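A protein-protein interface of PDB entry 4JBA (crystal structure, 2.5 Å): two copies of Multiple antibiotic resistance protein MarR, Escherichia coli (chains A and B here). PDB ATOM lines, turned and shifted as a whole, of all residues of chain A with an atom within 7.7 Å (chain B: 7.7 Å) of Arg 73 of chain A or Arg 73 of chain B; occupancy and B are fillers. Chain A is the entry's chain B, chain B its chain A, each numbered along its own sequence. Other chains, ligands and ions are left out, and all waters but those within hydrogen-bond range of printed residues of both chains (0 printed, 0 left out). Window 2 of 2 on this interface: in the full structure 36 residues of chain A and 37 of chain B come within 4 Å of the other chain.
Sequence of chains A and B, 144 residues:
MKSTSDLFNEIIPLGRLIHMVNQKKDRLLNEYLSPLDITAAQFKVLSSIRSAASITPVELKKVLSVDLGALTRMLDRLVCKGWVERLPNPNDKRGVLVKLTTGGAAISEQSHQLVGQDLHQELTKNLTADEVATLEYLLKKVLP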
ATOM      1  N   ASP A  67      20.152   1.517 -19.338  1.00  0.00           N
ATOM      2  CA  ASP A  67      19.858   0.141 -19.673  1.00  0.00           C
ATOM      3  C   ASP A  67      18.351  -0.126 -19.806  1.00  0.00           C
ATOM      4  O   ASP A  67      17.529   0.525 -19.151  1.00  0.00           O
ATOM      5  CB  ASP A  67      20.476  -0.804 -18.649  1.00  0.00           C
ATOM      6  CG  ASP A  67      20.367  -2.251 -19.063  1.00  0.00           C
ATOM      7  OD1 ASP A  67      20.731  -2.567 -20.216  1.00  0.00           O
ATOM      8  OD2 ASP A  67      19.863  -3.067 -18.260  1.00  0.00           O
ATOM      9  N   LEU A  68      18.010  -1.118 -20.629  1.00  0.00           N
ATOM     10  CA  LEU A  68      16.621  -1.451 -20.941  1.00  0.00           C
ATOM     11  C   LEU A  68      15.835  -1.850 -19.679  1.00  0.00           C
ATOM     12  O   LEU A  68      14.725  -1.363 -19.445  1.00  0.00           O
ATOM     13  CB  LEU A  68      16.579  -2.582 -21.979  1.00  0.00           C
ATOM     14  CG  LEU A  68      15.286  -2.875 -22.754  1.00  0.00           C
ATOM     15  CD1 LEU A  68      14.041  -2.489 -21.971  1.00  0.00           C
ATOM     16  CD2 LEU A  68      15.290  -2.252 -24.142  1.00  0.00           C
ATOM     17  N   GLY A  69      16.422  -2.726 -18.871  1.00  0.00           N
ATOM     18  CA  GLY A  69      15.804  -3.141 -17.613  1.00  0.00           C
ATOM     19  C   GLY A  69      15.559  -1.986 -16.652  1.00  0.00           C
ATOM     20  O   GLY A  69      14.472  -1.852 -16.096  1.00  0.00           O
ATOM     21  N   ALA A  70      16.579  -1.153 -16.456  1.00  0.00           N
ATOM     22  CA  ALA A  70      16.495  -0.024 -15.515  1.00  0.00           C
ATOM     23  C   ALA A  70      15.334   0.923 -15.843  1.00  0.00           C
ATOM     24  O   ALA A  70      14.758   1.553 -14.954  1.00  0.00           O
ATOM     25  CB  ALA A  70      17.815   0.742 -15.479  1.00  0.00           C
ATOM     26  N   LEU A  71      14.990   1.006 -17.119  1.00  0.00           N
ATOM     27  CA  LEU A  71      13.940   1.890 -17.563  1.00  0.00           C
ATOM     28  C   LEU A  71      12.554   1.281 -17.323  1.00  0.00           C
ATOM     29  O   LEU A  71      11.648   1.961 -16.824  1.00  0.00           O
ATOM     30  CB  LEU A  71      14.130   2.228 -19.035  1.00  0.00           C
ATOM     31  CG  LEU A  71      13.150   3.211 -19.666  1.00  0.00           C
ATOM     32  CD1 LEU A  71      13.170   4.544 -18.935  1.00  0.00           C
ATOM     33  CD2 LEU A  71      13.474   3.397 -21.140  1.00  0.00           C
ATOM     34  N   THR A  72      12.396   0.000 -17.674  1.00  0.00           N
ATOM     35  CA  THR A  72      11.189  -0.761 -17.323  1.00  0.00           C
ATOM     36  C   THR A  72      10.831  -0.584 -15.849  1.00  0.00           C
ATOM     37  O   THR A  72       9.693  -0.252 -15.510  1.00  0.00           O
ATOM     38  CB  THR A  72      11.359  -2.269 -17.615  1.00  0.00           C
ATOM     39  OG1 THR A  72      12.041  -2.448 -18.860  1.00  0.00           O
ATOM     40  CG2 THR A  72       9.999  -2.955 -17.685  1.00  0.00           C
ATOM     41  N   ARG A  73      11.812  -0.790 -14.978  1.00  0.00           N
ATOM     42  CA  ARG A  73      11.617  -0.591 -13.554  1.00  0.00           C
ATOM     43  C   ARG A  73      11.187   0.831 -13.243  1.00  0.00           C
ATOM     44  O   ARG A  73      10.250   1.048 -12.468  1.00  0.00           O
ATOM     45  CB  ARG A  73      12.889  -0.944 -12.780  1.00  0.00           C
ATOM     46  CG  ARG A  73      12.948  -2.397 -12.312  1.00  0.00           C
ATOM     47  CD  ARG A  73      14.269  -2.711 -11.621  1.00  0.00           C
ATOM     48  NE  ARG A  73      14.158  -2.666 -10.163  1.00  0.00           N
ATOM     49  CZ  ARG A  73      15.175  -2.867  -9.324  1.00  0.00           C
ATOM     50  NH1 ARG A  73      16.390  -3.121  -9.795  1.00  0.00           N
ATOM     51  NH2 ARG A  73      14.976  -2.812  -8.014  1.00  0.00           N
ATOM     52  N   MET A  74      11.868   1.802 -13.865  1.00  0.00           N
ATOM     53  CA  MET A  74      11.585   3.224 -13.640  1.00  0.00           C
ATOM     54  C   MET A  74      10.181   3.592 -14.105  1.00  0.00           C
ATOM     55  O   MET A  74       9.426   4.248 -13.381  1.00  0.00           O
ATOM     56  CB  MET A  74      12.613   4.090 -14.361  1.00  0.00           C
ATOM     57  CG  MET A  74      12.254   5.570 -14.416  1.00  0.00           C
ATOM     58  SD  MET A  74      13.415   6.621 -13.513  1.00  0.00           S
ATOM     59  CE  MET A  74      14.953   6.271 -14.381  1.00  0.00           C
ATOM     60  N   LEU A  75       9.835   3.163 -15.314  1.00  0.00           N
ATOM     61  CA  LEU A  75       8.465   3.263 -15.809  1.00  0.00           C
ATOM     62  C   LEU A  75       7.428   2.626 -14.862  1.00  0.00           C
ATOM     63  O   LEU A  75       6.351   3.191 -14.648  1.00  0.00           O
ATOM     64  CB  LEU A  75       8.358   2.647 -17.202  1.00  0.00           C
ATOM     65  CG  LEU A  75       9.232   3.330 -18.254  1.00  0.00           C
ATOM     66  CD1 LEU A  75       9.336   2.490 -19.514  1.00  0.00           C
ATOM     67  CD2 LEU A  75       8.684   4.711 -18.571  1.00  0.00           C
ATOM     68  N   ASP A  76       7.761   1.469 -14.288  1.00  0.00           N
ATOM     69  CA  ASP A  76       6.875   0.831 -13.307  1.00  0.00           C
ATOM     70  C   ASP A  76       6.529   1.796 -12.193  1.00  0.00           C
ATOM     71  O   ASP A  76       5.356   1.995 -11.875  1.00  0.00           O
ATOM     72  CB  ASP A  76       7.516  -0.433 -12.724  1.00  0.00           C
ATOM     73  CG  ASP A  76       7.342  -1.634 -13.619  1.00  0.00           C
ATOM     74  OD1 ASP A  76       6.517  -1.557 -14.556  1.00  0.00           O
ATOM     75  OD2 ASP A  76       8.044  -2.651 -13.399  1.00  0.00           O
ATOM     76  N   ARG A  77       7.561   2.405 -11.607  1.00  0.00           N
ATOM     77  CA  ARG A  77       7.376   3.384 -10.536  1.00  0.00           C
ATOM     78  C   ARG A  77       6.553   4.591 -11.017  1.00  0.00           C
ATOM     79  O   ARG A  77       5.575   4.989 -10.367  1.00  0.00           O
ATOM     80  CB  ARG A  77       8.733   3.850  -9.992  1.00  0.00           C
ATOM     81  CG  ARG A  77       9.304   2.971  -8.885  1.00  0.00           C
ATOM     82  CD  ARG A  77      10.647   3.505  -8.390  1.00  0.00           C
ATOM     83  NE  ARG A  77      11.765   3.021  -9.202  1.00  0.00           N
ATOM     84  CZ  ARG A  77      12.605   2.059  -8.824  1.00  0.00           C
ATOM     85  NH1 ARG A  77      12.477   1.491  -7.630  1.00  0.00           N
ATOM     86  NH2 ARG A  77      13.583   1.677  -9.633  1.00  0.00           N
ATOM     87  N   LEU A  78       6.937   5.150 -12.167  1.00  0.00           N
ATOM     88  CA  LEU A  78       6.260   6.324 -12.706  1.00  0.00           C
ATOM     89  C   LEU A  78       4.789   6.049 -12.944  1.00  0.00           C
ATOM     90  O   LEU A  78       3.939   6.890 -12.644  1.00  0.00           O
ATOM     91  CB  LEU A  78       6.926   6.793 -13.998  1.00  0.00           C
ATOM     92  CG  LEU A  78       8.384   7.273 -13.878  1.00  0.00           C
ATOM     93  CD1 LEU A  78       8.940   7.654 -15.238  1.00  0.00           C
ATOM     94  CD2 LEU A  78       8.502   8.428 -12.908  1.00  0.00           C
ATOM     95  N   VAL A  79       4.488   4.861 -13.475  1.00  0.00           N
ATOM     96  CA  VAL A  79       3.105   4.415 -13.634  1.00  0.00           C
ATOM     97  C   VAL A  79       2.378   4.335 -12.289  1.00  0.00           C
ATOM     98  O   VAL A  79       1.259   4.819 -12.158  1.00  0.00           O
ATOM     99  CB  VAL A  79       3.022   3.036 -14.342  1.00  0.00           C
ATOM    100  CG1 VAL A  79       1.630   2.459 -14.218  1.00  0.00           C
ATOM    101  CG2 VAL A  79       3.414   3.164 -15.804  1.00  0.00           C
ATOM    102  N   ARG A  86       0.948   3.086 -19.671  1.00  0.00           N
ATOM    103  CA  ARG A  86       1.298   2.200 -20.782  1.00  0.00           C
ATOM    104  C   ARG A  86       0.113   2.036 -21.737  1.00  0.00           C
ATOM    105  O   ARG A  86      -1.041   2.142 -21.328  1.00  0.00           O
ATOM    106  CB  ARG A  86       1.756   0.832 -20.260  1.00  0.00           C
ATOM    107  CG  ARG A  86       3.081   0.858 -19.500  1.00  0.00           C
ATOM    108  CD  ARG A  86       3.297  -0.435 -18.715  1.00  0.00           C
ATOM    109  NE  ARG A  86       4.567  -0.448 -17.976  1.00  0.00           N
ATOM    110  CZ  ARG A  86       5.771  -0.563 -18.544  1.00  0.00           C
ATOM    111  NH1 ARG A  86       5.886  -0.615 -19.867  1.00  0.00           N
ATOM    112  NH2 ARG A  86       6.865  -0.599 -17.789  1.00  0.00           N
ATOM    113  N   ASP B  67      19.883   5.152  -9.597  1.00  0.00           N
ATOM    114  CA  ASP B  67      19.138   4.497  -8.516  1.00  0.00           C
ATOM    115  C   ASP B  67      19.923   3.334  -7.895  1.00  0.00           C
ATOM    116  O   ASP B  67      20.791   2.742  -8.542  1.00  0.00           O
ATOM    117  CB  ASP B  67      17.775   4.014  -9.015  1.00  0.00           C
ATOM    118  CG  ASP B  67      16.866   3.573  -7.886  1.00  0.00           C
ATOM    119  OD1 ASP B  67      16.750   4.318  -6.889  1.00  0.00           O
ATOM    120  OD2 ASP B  67      16.280   2.477  -7.987  1.00  0.00           O
ATOM    121  N   LEU B  68      19.606   3.010  -6.640  1.00  0.00           N
ATOM    122  CA  LEU B  68      20.359   1.999  -5.893  1.00  0.00           C
ATOM    123  C   LEU B  68      20.152   0.592  -6.440  1.00  0.00           C
ATOM    124  O   LEU B  68      21.102  -0.186  -6.541  1.00  0.00           O
ATOM    125  CB  LEU B  68      20.006   2.036  -4.408  1.00  0.00           C
ATOM    126  CG  LEU B  68      21.112   1.459  -3.510  1.00  0.00           C
ATOM    127  CD1 LEU B  68      21.176   2.159  -2.163  1.00  0.00           C
ATOM    128  CD2 LEU B  68      20.994  -0.056  -3.357  1.00  0.00           C
ATOM    129  N   GLY B  69      18.899   0.254  -6.738  1.00  0.00           N
ATOM    130  CA  GLY B  69      18.570  -1.031  -7.348  1.00  0.00           C
ATOM    131  C   GLY B  69      19.248  -1.231  -8.690  1.00  0.00           C
ATOM    132  O   GLY B  69      19.867  -2.267  -8.930  1.00  0.00           O
ATOM    133  N   ALA B  70      19.153  -0.220  -9.557  1.00  0.00           N
ATOM    134  CA  ALA B  70      19.742  -0.280 -10.901  1.00  0.00           C
ATOM    135  C   ALA B  70      21.238  -0.592 -10.851  1.00  0.00           C
ATOM    136  O   ALA B  70      21.771  -1.262 -11.736  1.00  0.00           O
ATOM    137  CB  ALA B  70      19.495   1.025 -11.652  1.00  0.00           C
ATOM    138  N   LEU B  71      21.905  -0.109  -9.805  1.00  0.00           N
ATOM    139  CA  LEU B  71      23.337  -0.305  -9.647  1.00  0.00           C
ATOM    140  C   LEU B  71      23.671  -1.716  -9.160  1.00  0.00           C
ATOM    141  O   LEU B  71      24.621  -2.337  -9.643  1.00  0.00           O
ATOM    142  CB  LEU B  71      23.910   0.737  -8.686  1.00  0.00           C
ATOM    143  CG  LEU B  71      25.393   0.615  -8.346  1.00  0.00           C
ATOM    144  CD1 LEU B  71      26.247   0.881  -9.575  1.00  0.00           C
ATOM    145  CD2 LEU B  71      25.753   1.565  -7.221  1.00  0.00           C
ATOM    146  N   THR B  72      22.903  -2.206  -8.187  1.00  0.00           N
ATOM    147  CA  THR B  72      22.980  -3.612  -7.771  1.00  0.00           C
ATOM    148  C   THR B  72      22.879  -4.572  -8.968  1.00  0.00           C
ATOM    149  O   THR B  72      23.684  -5.498  -9.100  1.00  0.00           O
ATOM    150  CB  THR B  72      21.884  -3.961  -6.747  1.00  0.00           C
ATOM    151  OG1 THR B  72      21.787  -2.911  -5.773  1.00  0.00           O
ATOM    152  CG2 THR B  72      22.207  -5.276  -6.041  1.00  0.00           C
ATOM    153  N   ARG B  73      21.896  -4.337  -9.840  1.00  0.00           N
ATOM    154  CA  ARG B  73      21.745  -5.129 -11.070  1.00  0.00           C
ATOM    155  C   ARG B  73      22.965  -4.983 -11.964  1.00  0.00           C
ATOM    156  O   ARG B  73      23.445  -5.960 -12.539  1.00  0.00           O
ATOM    157  CB  ARG B  73      20.485  -4.708 -11.840  1.00  0.00           C
ATOM    158  CG  ARG B  73      19.219  -5.442 -11.429  1.00  0.00           C
ATOM    159  CD  ARG B  73      18.006  -4.933 -12.200  1.00  0.00           C
ATOM    160  NE  ARG B  73      17.695  -5.769 -13.368  1.00  0.00           N
ATOM    161  CZ  ARG B  73      16.647  -5.581 -14.175  1.00  0.00           C
ATOM    162  NH1 ARG B  73      15.800  -4.586 -13.953  1.00  0.00           N
ATOM    163  NH2 ARG B  73      16.450  -6.391 -15.209  1.00  0.00           N
ATOM    164  N   MET B  74      23.456  -3.753 -12.082  1.00  0.00           N
ATOM    165  CA  MET B  74      24.607  -3.455 -12.922  1.00  0.00           C
ATOM    166  C   MET B  74      25.842  -4.157 -12.394  1.00  0.00           C
ATOM    167  O   MET B  74      26.589  -4.777 -13.153  1.00  0.00           O
ATOM    168  CB  MET B  74      24.845  -1.950 -12.981  1.00  0.00           C
ATOM    169  CG  MET B  74      26.116  -1.546 -13.711  1.00  0.00           C
ATOM    170  SD  MET B  74      25.797  -0.686 -15.265  1.00  0.00           S
ATOM    171  CE  MET B  74      24.982   0.799 -14.674  1.00  0.00           C
ATOM    172  N   LEU B  75      26.038  -4.087 -11.084  1.00  0.00           N
ATOM    173  CA  LEU B  75      27.146  -4.773 -10.440  1.00  0.00           C
ATOM    174  C   LEU B  75      27.048  -6.284 -10.631  1.00  0.00           C
ATOM    175  O   LEU B  75      28.046  -6.948 -10.933  1.00  0.00           O
ATOM    176  CB  LEU B  75      27.208  -4.419  -8.951  1.00  0.00           C
ATOM    177  CG  LEU B  75      27.538  -2.952  -8.618  1.00  0.00           C
ATOM    178  CD1 LEU B  75      27.287  -2.639  -7.147  1.00  0.00           C
ATOM    179  CD2 LEU B  75      28.967  -2.597  -9.005  1.00  0.00           C
ATOM    180  N   ASP B  76      25.833  -6.817 -10.503  1.00  0.00           N
ATOM    181  CA  ASP B  76      25.582  -8.229 -10.788  1.00  0.00           C
ATOM    182  C   ASP B  76      26.156  -8.635 -12.136  1.00  0.00           C
ATOM    183  O   ASP B  76      26.922  -9.595 -12.230  1.00  0.00           O
ATOM    184  CB  ASP B  76      24.085  -8.534 -10.741  1.00  0.00           C
ATOM    185  CG  ASP B  76      23.574  -8.739  -9.325  1.00  0.00           C
ATOM    186  OD1 ASP B  76      24.403  -8.900  -8.406  1.00  0.00           O
ATOM    187  OD2 ASP B  76      22.344  -8.736  -9.131  1.00  0.00           O
ATOM    188  N   ARG B  77      25.796  -7.888 -13.177  1.00  0.00           N
ATOM    189  CA  ARG B  77      26.312  -8.137 -14.518  1.00  0.00           C
ATOM    190  C   ARG B  77      27.840  -8.024 -14.574  1.00  0.00           C
ATOM    191  O   ARG B  77      28.512  -8.873 -15.169  1.00  0.00           O
ATOM    192  CB  ARG B  77      25.678  -7.179 -15.518  1.00  0.00           C
ATOM    193  CG  ARG B  77      24.422  -7.710 -16.177  1.00  0.00           C
ATOM    194  CD  ARG B  77      23.814  -6.685 -17.116  1.00  0.00           C
ATOM    195  NE  ARG B  77      23.029  -5.693 -16.392  1.00  0.00           N
ATOM    196  CZ  ARG B  77      21.703  -5.621 -16.419  1.00  0.00           C
ATOM    197  NH1 ARG B  77      21.000  -6.468 -17.162  1.00  0.00           N
ATOM    198  NH2 ARG B  77      21.077  -4.686 -15.718  1.00  0.00           N
ATOM    199  N   LEU B  78      28.383  -6.973 -13.951  1.00  0.00           N
ATOM    200  CA  LEU B  78      29.823  -6.708 -14.001  1.00  0.00           C
ATOM    201  C   LEU B  78      30.612  -7.795 -13.290  1.00  0.00           C
ATOM    202  O   LEU B  78      31.707  -8.161 -13.717  1.00  0.00           O
ATOM    203  CB  LEU B  78      30.144  -5.345 -13.397  1.00  0.00           C
ATOM    204  CG  LEU B  78      29.525  -4.128 -14.091  1.00  0.00           C
ATOM    205  CD1 LEU B  78      29.834  -2.865 -13.312  1.00  0.00           C
ATOM    206  CD2 LEU B  78      30.001  -4.011 -15.534  1.00  0.00           C
ATOM    207  N   VAL B  79      30.043  -8.315 -12.210  1.00  0.00           N
ATOM    208  CA  VAL B  79      30.624  -9.447 -11.508  1.00  0.00           C
ATOM    209  C   VAL B  79      30.608 -10.704 -12.374  1.00  0.00           C
ATOM    210  O   VAL B  79      31.596 -11.423 -12.446  1.00  0.00           O
ATOM    211  CB  VAL B  79      29.895  -9.718 -10.182  1.00  0.00           C
ATOM    212  CG1 VAL B  79      30.198 -11.118  -9.681  1.00  0.00           C
ATOM    213  CG2 VAL B  79      30.290  -8.685  -9.147  1.00  0.00           C
ATOM    214  N   ARG B  86      32.770  -8.605  -5.389  1.00  0.00           N
ATOM    215  CA  ARG B  86      32.239  -8.166  -4.100  1.00  0.00           C
ATOM    216  C   ARG B  86      33.127  -8.658  -2.950  1.00  0.00           C
ATOM    217  O   ARG B  86      33.769  -9.709  -3.053  1.00  0.00           O
ATOM    218  CB  ARG B  86      30.801  -8.677  -3.909  1.00  0.00           C
ATOM    219  CG  ARG B  86      29.781  -8.077  -4.870  1.00  0.00           C
ATOM    220  CD  ARG B  86      28.459  -8.841  -4.822  1.00  0.00           C
ATOM    221  NE  ARG B  86      27.457  -8.289  -5.739  1.00  0.00           N
ATOM    222  CZ  ARG B  86      26.754  -7.179  -5.509  1.00  0.00           C
ATOM    223  NH1 ARG B  86      26.962  -6.471  -4.401  1.00  0.00           N
ATOM    224  NH2 ARG B  86      25.853  -6.768  -6.396  1.00  0.00           N
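OD2 of Asp 67 of chain B is in salt-bridge range of NH2 of Arg 77 of chain A.
The guanidinium group (NH2) of Arg 77 of chain B lies within salt-bridge range of the side-chain carboxylate (OD2) of Asp 67 of chain A, at 3.2 Å.
Gly 69 of chain A touches Arg 73 of chain B (O to NH1, 3.7 Å).
Gly 69 of chain B touches Arg 73 of chain A.
Arg 73 of chain B touches Arg 73 of chain A.
Of the printed residues of chain B, Arg 73 of chain A touches Gly 69 (3.6 Å) and Arg 73 (3.4 Å).
Of the printed residues of chain B, Arg 77 of chain A touches Asp 67 (3.3 Å).
Arg 86 of chain A touches none of the printed residues of chain B.
Printed residues of chain A within 4 Å of Asp 67 of chain B: Arg 77 (3.3 Å).
Arg 73 of chain B touches just these residues of chain A: Gly 69 and Arg 73.
Asp 76 of chain B touches none of the printed residues of chain A.
Of the printed residues of chain A, Arg 77 of chain B touches Asp 67.
The nearest printed residue of chain B that does not touch Arg 73 of chain A is Ala 70 of chain B (4.01 Å).
The nearest residue of chain A that does not touch Arg 73 of chain B is Ala 70 of chain A (4.3 Å).
The nearest printed residue of chain B that does not touch Gly 69 of chain A is Arg 77 of chain B (5.8 Å).
Of the 14 printed residues of chain B, 4 touch a printed residue of chain A.
Along chain A the printed residues that touch a printed residue of chain B span positions 67 to 77.
Asp 67 of chain A touches Arg 77 of chain B, and with the chains exchanged Arg 77 of chain A touches Asp 67 of chain B.
Gly 69 of chain A touches Arg 73 of chain B, and with the chains exchanged Arg 73 of chain A touches Gly 69 of chain B.
Arg 73 of chain B touches its own counterpart, Arg 73 of chain A.
14 positions are printed for both chains.
Of the 5 pairs that touch across the chains among the printed residues, 5 have their exchanged pair printed and touching as well.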
